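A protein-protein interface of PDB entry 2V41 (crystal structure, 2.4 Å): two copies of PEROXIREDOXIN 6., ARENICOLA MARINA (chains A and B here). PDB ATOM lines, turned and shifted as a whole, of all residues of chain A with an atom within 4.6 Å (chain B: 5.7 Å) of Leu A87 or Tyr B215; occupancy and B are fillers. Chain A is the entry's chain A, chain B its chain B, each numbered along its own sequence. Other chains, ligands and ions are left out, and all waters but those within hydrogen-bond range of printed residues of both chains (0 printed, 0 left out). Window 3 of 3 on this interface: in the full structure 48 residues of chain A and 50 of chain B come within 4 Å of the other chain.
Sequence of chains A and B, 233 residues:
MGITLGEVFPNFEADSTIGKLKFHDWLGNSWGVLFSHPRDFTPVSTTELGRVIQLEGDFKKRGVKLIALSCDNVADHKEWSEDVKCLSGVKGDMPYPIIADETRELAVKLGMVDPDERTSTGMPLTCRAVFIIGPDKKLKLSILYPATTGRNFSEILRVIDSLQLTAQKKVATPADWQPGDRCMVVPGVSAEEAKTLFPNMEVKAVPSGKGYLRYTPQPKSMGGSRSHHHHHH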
ATOM      1  N   THR A  46       4.478   6.180 -25.186  1.00  0.00           N
ATOM      2  CA  THR A  46       4.663   4.979 -24.324  1.00  0.00           C
ATOM      3  C   THR A  46       3.728   3.801 -24.716  1.00  0.00           C
ATOM      4  O   THR A  46       4.123   2.617 -24.700  1.00  0.00           O
ATOM      5  CB  THR A  46       4.502   5.327 -22.805  1.00  0.00           C
ATOM      6  OG1 THR A  46       5.289   6.479 -22.472  1.00  0.00           O
ATOM      7  CG2 THR A  46       4.958   4.211 -21.923  1.00  0.00           C
ATOM      8  N   THR A  47       2.490   4.128 -25.066  1.00  0.00           N
ATOM      9  CA  THR A  47       1.540   3.142 -25.547  1.00  0.00           C
ATOM     10  C   THR A  47       2.060   2.558 -26.853  1.00  0.00           C
ATOM     11  O   THR A  47       2.049   1.357 -27.008  1.00  0.00           O
ATOM     12  CB  THR A  47       0.065   3.704 -25.671  1.00  0.00           C
ATOM     13  OG1 THR A  47      -0.021   4.682 -26.728  1.00  0.00           O
ATOM     14  CG2 THR A  47      -0.417   4.298 -24.338  1.00  0.00           C
ATOM     15  N   ASP A  83       9.491   2.415 -18.224  1.00  0.00           N
ATOM     16  CA  ASP A  83       8.062   2.689 -18.269  1.00  0.00           C
ATOM     17  C   ASP A  83       7.398   2.011 -19.504  1.00  0.00           C
ATOM     18  O   ASP A  83       6.291   1.478 -19.387  1.00  0.00           O
ATOM     19  CB  ASP A  83       7.793   4.191 -18.385  1.00  0.00           C
ATOM     20  CG  ASP A  83       8.369   4.996 -17.278  1.00  0.00           C
ATOM     21  OD1 ASP A  83       8.771   4.457 -16.242  1.00  0.00           O
ATOM     22  OD2 ASP A  83       8.359   6.218 -17.440  1.00  0.00           O
ATOM     23  N   VAL A  84       8.039   2.078 -20.672  1.00  0.00           N
ATOM     24  CA  VAL A  84       7.532   1.376 -21.848  1.00  0.00           C
ATOM     25  C   VAL A  84       7.403  -0.132 -21.596  1.00  0.00           C
ATOM     26  O   VAL A  84       6.355  -0.718 -21.878  1.00  0.00           O
ATOM     27  CB  VAL A  84       8.419   1.578 -23.104  1.00  0.00           C
ATOM     28  CG1 VAL A  84       7.948   0.656 -24.218  1.00  0.00           C
ATOM     29  CG2 VAL A  84       8.436   3.022 -23.540  1.00  0.00           C
ATOM     30  N   LYS A  85       8.472  -0.745 -21.064  1.00  0.00           N
ATOM     31  CA  LYS A  85       8.472  -2.167 -20.615  1.00  0.00           C
ATOM     32  C   LYS A  85       7.263  -2.511 -19.708  1.00  0.00           C
ATOM     33  O   LYS A  85       6.563  -3.519 -19.885  1.00  0.00           O
ATOM     34  CB  LYS A  85       9.747  -2.496 -19.810  1.00  0.00           C
ATOM     35  CG  LYS A  85      11.063  -2.472 -20.591  1.00  0.00           C
ATOM     36  CD  LYS A  85      12.204  -3.002 -19.734  1.00  0.00           C
ATOM     37  CE  LYS A  85      13.429  -3.207 -20.575  1.00  0.00           C
ATOM     38  NZ  LYS A  85      14.675  -3.416 -19.799  1.00  0.00           N
ATOM     39  N   CYS A  86       7.048  -1.664 -18.720  1.00  0.00           N
ATOM     40  CA  CYS A  86       5.989  -1.871 -17.742  1.00  0.00           C
ATOM     41  C   CYS A  86       4.594  -1.730 -18.381  1.00  0.00           C
ATOM     42  O   CYS A  86       3.748  -2.582 -18.180  1.00  0.00           O
ATOM     43  CB  CYS A  86       6.200  -0.884 -16.591  1.00  0.00           C
ATOM     44  SG  CYS A  86       4.845  -0.730 -15.450  1.00  0.00           S
ATOM     45  N   LEU A  87       4.359  -0.691 -19.191  1.00  0.00           N
ATOM     46  CA  LEU A  87       3.066  -0.603 -19.948  1.00  0.00           C
ATOM     47  C   LEU A  87       2.835  -1.862 -20.767  1.00  0.00           C
ATOM     48  O   LEU A  87       1.735  -2.350 -20.772  1.00  0.00           O
ATOM     49  CB  LEU A  87       2.989   0.592 -20.901  1.00  0.00           C
ATOM     50  CG  LEU A  87       1.662   1.409 -21.036  1.00  0.00           C
ATOM     51  CD1 LEU A  87       1.479   1.849 -22.479  1.00  0.00           C
ATOM     52  CD2 LEU A  87       0.362   0.766 -20.562  1.00  0.00           C
ATOM     53  N   SER A  88       3.886  -2.363 -21.439  1.00  0.00           N
ATOM     54  CA  SER A  88       3.812  -3.507 -22.369  1.00  0.00           C
ATOM     55  C   SER A  88       3.283  -4.815 -21.778  1.00  0.00           C
ATOM     56  O   SER A  88       2.565  -5.541 -22.472  1.00  0.00           O
ATOM     57  CB  SER A  88       5.191  -3.780 -23.008  1.00  0.00           C
ATOM     58  OG  SER A  88       6.121  -4.455 -22.163  1.00  0.00           O
ATOM     59  N   GLY A  89       3.619  -5.079 -20.504  1.00  0.00           N
ATOM     60  CA  GLY A  89       3.276  -6.327 -19.825  1.00  0.00           C
ATOM     61  C   GLY A  89       4.331  -7.435 -19.975  1.00  0.00           C
ATOM     62  O   GLY A  89       4.268  -8.484 -19.279  1.00  0.00           O
ATOM     63  N   ARG B 182     -10.491   5.455 -24.704  1.00  0.00           N
ATOM     64  CA  ARG B 182      -9.962   6.538 -23.916  1.00  0.00           C
ATOM     65  C   ARG B 182      -8.766   7.164 -24.612  1.00  0.00           C
ATOM     66  O   ARG B 182      -8.001   6.491 -25.319  1.00  0.00           O
ATOM     67  CB  ARG B 182      -9.499   6.071 -22.525  1.00  0.00           C
ATOM     68  CG  ARG B 182     -10.500   5.310 -21.724  1.00  0.00           C
ATOM     69  CD  ARG B 182     -10.068   5.287 -20.254  1.00  0.00           C
ATOM     70  NE  ARG B 182      -8.968   4.357 -19.968  1.00  0.00           N
ATOM     71  CZ  ARG B 182      -8.367   4.239 -18.782  1.00  0.00           C
ATOM     72  NH1 ARG B 182      -8.746   5.016 -17.783  1.00  0.00           N
ATOM     73  NH2 ARG B 182      -7.375   3.371 -18.616  1.00  0.00           N
ATOM     74  N   CYS B 183      -8.587   8.456 -24.366  1.00  0.00           N
ATOM     75  CA  CYS B 183      -7.534   9.203 -24.979  1.00  0.00           C
ATOM     76  C   CYS B 183      -6.526   9.562 -23.916  1.00  0.00           C
ATOM     77  O   CYS B 183      -6.802   9.368 -22.721  1.00  0.00           O
ATOM     78  CB  CYS B 183      -8.118  10.475 -25.546  1.00  0.00           C
ATOM     79  SG  CYS B 183      -9.287  10.125 -26.738  1.00  0.00           S
ATOM     80  N   MET B 184      -5.389  10.109 -24.343  1.00  0.00           N
ATOM     81  CA  MET B 184      -4.396  10.532 -23.413  1.00  0.00           C
ATOM     82  C   MET B 184      -4.513  12.026 -23.262  1.00  0.00           C
ATOM     83  O   MET B 184      -4.827  12.703 -24.211  1.00  0.00           O
ATOM     84  CB  MET B 184      -2.991  10.145 -23.897  1.00  0.00           C
ATOM     85  CG  MET B 184      -2.863   8.706 -24.310  1.00  0.00           C
ATOM     86  SD  MET B 184      -3.505   7.465 -23.165  1.00  0.00           S
ATOM     87  CE  MET B 184      -2.312   7.553 -21.817  1.00  0.00           C
ATOM     88  N   VAL B 185      -4.315  12.529 -22.050  1.00  0.00           N
ATOM     89  CA  VAL B 185      -4.325  13.970 -21.809  1.00  0.00           C
ATOM     90  C   VAL B 185      -2.939  14.363 -22.226  1.00  0.00           C
ATOM     91  O   VAL B 185      -1.964  13.703 -21.825  1.00  0.00           O
ATOM     92  CB  VAL B 185      -4.563  14.293 -20.334  1.00  0.00           C
ATOM     93  CG1 VAL B 185      -4.399  15.760 -20.038  1.00  0.00           C
ATOM     94  CG2 VAL B 185      -5.937  13.769 -19.936  1.00  0.00           C
ATOM     95  N   ASN B 200     -12.305  13.266 -14.870  1.00  0.00           N
ATOM     96  CA  ASN B 200     -12.374  11.795 -14.806  1.00  0.00           C
ATOM     97  C   ASN B 200     -11.083  11.134 -15.231  1.00  0.00           C
ATOM     98  O   ASN B 200     -11.016   9.945 -15.442  1.00  0.00           O
ATOM     99  CB  ASN B 200     -13.552  11.278 -15.647  1.00  0.00           C
ATOM    100  CG  ASN B 200     -14.879  11.959 -15.271  1.00  0.00           C
ATOM    101  OD1 ASN B 200     -15.281  11.982 -14.089  1.00  0.00           O
ATOM    102  ND2 ASN B 200     -15.549  12.541 -16.274  1.00  0.00           N
ATOM    103  N   MET B 201     -10.041  11.927 -15.322  1.00  0.00           N
ATOM    104  CA  MET B 201      -8.725  11.433 -15.650  1.00  0.00           C
ATOM    105  C   MET B 201      -8.196  10.509 -14.532  1.00  0.00           C
ATOM    106  O   MET B 201      -8.459  10.698 -13.359  1.00  0.00           O
ATOM    107  CB  MET B 201      -7.812  12.642 -15.866  1.00  0.00           C
ATOM    108  CG  MET B 201      -6.353  12.380 -16.176  1.00  0.00           C
ATOM    109  SD  MET B 201      -5.431  13.887 -15.742  1.00  0.00           S
ATOM    110  CE  MET B 201      -5.909  14.920 -17.116  1.00  0.00           C
ATOM    111  N   GLU B 202      -7.488   9.485 -14.978  1.00  0.00           N
ATOM    112  CA  GLU B 202      -6.701   8.575 -14.204  1.00  0.00           C
ATOM    113  C   GLU B 202      -5.260   8.842 -14.585  1.00  0.00           C
ATOM    114  O   GLU B 202      -4.904   8.794 -15.747  1.00  0.00           O
ATOM    115  CB  GLU B 202      -7.055   7.130 -14.598  1.00  0.00           C
ATOM    116  CG  GLU B 202      -5.927   6.051 -14.304  1.00  0.00           C
ATOM    117  CD  GLU B 202      -6.168   4.631 -14.910  1.00  0.00           C
ATOM    118  OE1 GLU B 202      -6.709   4.508 -16.039  1.00  0.00           O
ATOM    119  OE2 GLU B 202      -5.753   3.645 -14.255  1.00  0.00           O
ATOM    120  N   VAL B 203      -4.441   9.136 -13.589  1.00  0.00           N
ATOM    121  CA  VAL B 203      -2.990   9.022 -13.677  1.00  0.00           C
ATOM    122  C   VAL B 203      -2.603   7.579 -13.316  1.00  0.00           C
ATOM    123  O   VAL B 203      -2.825   7.114 -12.208  1.00  0.00           O
ATOM    124  CB  VAL B 203      -2.276   9.969 -12.685  1.00  0.00           C
ATOM    125  CG1 VAL B 203      -0.799  10.059 -13.019  1.00  0.00           C
ATOM    126  CG2 VAL B 203      -2.963  11.358 -12.649  1.00  0.00           C
ATOM    127  N   LYS B 204      -2.039   6.876 -14.277  1.00  0.00           N
ATOM    128  CA  LYS B 204      -1.496   5.543 -14.052  1.00  0.00           C
ATOM    129  C   LYS B 204       0.006   5.665 -13.769  1.00  0.00           C
ATOM    130  O   LYS B 204       0.766   6.305 -14.529  1.00  0.00           O
ATOM    131  CB  LYS B 204      -1.774   4.660 -15.273  1.00  0.00           C
ATOM    132  CG  LYS B 204      -1.178   3.265 -15.226  1.00  0.00           C
ATOM    133  CD  LYS B 204      -1.401   2.486 -16.579  1.00  0.00           C
ATOM    134  CE  LYS B 204      -0.607   1.135 -16.586  1.00  0.00           C
ATOM    135  NZ  LYS B 204       0.327   1.017 -15.345  1.00  0.00           N
ATOM    136  N   LEU B 213       1.388   9.547 -17.688  1.00  0.00           N
ATOM    137  CA  LEU B 213       0.497   8.538 -18.305  1.00  0.00           C
ATOM    138  C   LEU B 213      -0.938   8.727 -17.871  1.00  0.00           C
ATOM    139  O   LEU B 213      -1.457   8.036 -17.011  1.00  0.00           O
ATOM    140  CB  LEU B 213       0.983   7.125 -18.011  1.00  0.00           C
ATOM    141  CG  LEU B 213       0.508   6.029 -18.975  1.00  0.00           C
ATOM    142  CD1 LEU B 213       0.971   6.260 -20.418  1.00  0.00           C
ATOM    143  CD2 LEU B 213       1.005   4.714 -18.436  1.00  0.00           C
ATOM    144  N   ARG B 214      -1.586   9.703 -18.473  1.00  0.00           N
ATOM    145  CA  ARG B 214      -2.885  10.137 -18.009  1.00  0.00           C
ATOM    146  C   ARG B 214      -3.920   9.860 -19.069  1.00  0.00           C
ATOM    147  O   ARG B 214      -3.781  10.301 -20.184  1.00  0.00           O
ATOM    148  CB  ARG B 214      -2.849  11.619 -17.677  1.00  0.00           C
ATOM    149  CG  ARG B 214      -1.816  11.980 -16.639  1.00  0.00           C
ATOM    150  CD  ARG B 214      -1.812  13.459 -16.319  1.00  0.00           C
ATOM    151  NE  ARG B 214      -1.497  14.270 -17.468  1.00  0.00           N
ATOM    152  CZ  ARG B 214      -1.482  15.596 -17.468  1.00  0.00           C
ATOM    153  NH1 ARG B 214      -1.756  16.279 -16.356  1.00  0.00           N
ATOM    154  NH2 ARG B 214      -1.170  16.241 -18.591  1.00  0.00           N
ATOM    155  N   TYR B 215      -4.934   9.104 -18.679  1.00  0.00           N
ATOM    156  CA  TYR B 215      -6.050   8.685 -19.507  1.00  0.00           C
ATOM    157  C   TYR B 215      -7.324   9.381 -19.080  1.00  0.00           C
ATOM    158  O   TYR B 215      -7.564   9.610 -17.853  1.00  0.00           O
ATOM    159  CB  TYR B 215      -6.336   7.220 -19.275  1.00  0.00           C
ATOM    160  CG  TYR B 215      -5.236   6.222 -19.609  1.00  0.00           C
ATOM    161  CD1 TYR B 215      -4.266   5.838 -18.654  1.00  0.00           C
ATOM    162  CD2 TYR B 215      -5.226   5.595 -20.858  1.00  0.00           C
ATOM    163  CE1 TYR B 215      -3.289   4.863 -18.971  1.00  0.00           C
ATOM    164  CE2 TYR B 215      -4.270   4.620 -21.172  1.00  0.00           C
ATOM    165  CZ  TYR B 215      -3.314   4.268 -20.244  1.00  0.00           C
ATOM    166  OH  TYR B 215      -2.428   3.322 -20.649  1.00  0.00           O
ATOM    167  N   THR B 216      -8.149   9.676 -20.093  1.00  0.00           N
ATOM    168  CA  THR B 216      -9.456  10.294 -19.899  1.00  0.00           C
ATOM    169  C   THR B 216     -10.465   9.679 -20.876  1.00  0.00           C
ATOM    170  O   THR B 216     -10.086   9.259 -21.945  1.00  0.00           O
ATOM    171  CB  THR B 216      -9.362  11.839 -20.089  1.00  0.00           C
ATOM    172  OG1 THR B 216     -10.625  12.451 -19.781  1.00  0.00           O
ATOM    173  CG2 THR B 216      -8.882  12.238 -21.529  1.00  0.00           C
ATOM    174  N   PRO B 217     -11.753   9.601 -20.497  1.00  0.00           N
ATOM    175  CA  PRO B 217     -12.710   9.158 -21.509  1.00  0.00           C
ATOM    176  C   PRO B 217     -12.636   9.989 -22.799  1.00  0.00           C
ATOM    177  O   PRO B 217     -12.120  11.097 -22.797  1.00  0.00           O
ATOM    178  CB  PRO B 217     -14.063   9.332 -20.817  1.00  0.00           C
ATOM    179  CG  PRO B 217     -13.755   9.187 -19.387  1.00  0.00           C
ATOM    180  CD  PRO B 217     -12.392   9.832 -19.200  1.00  0.00           C
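N of Glu B202 is in hydrogen-bond range of O of Tyr B215 (2.9 Å).
No position is printed for both chains.
Of the 14 printed residues of chain B, 1 touches a printed residue of chain A.
Of the 9 printed residues of chain A, 1 touches a printed residue of chain B.
Hydrophobic or aromatic side chains of chain A that line the printed part of chain B: Leu A87.
Of chain B, only Tyr B215 (3.8 Å) comes within 4 Å of Leu A87.
Tyr B215 touches just one residue of chain A: Leu A87.
Thr B216 touches none of the printed residues of chain A.
Asn B200 touches none of the printed residues of chain A.
The nearest residue of chain B that does not touch Leu A87 is Lys B204 (4.1 Å).
Among the printed residues, merely in contact across the chains: Leu A87 with Tyr B215.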
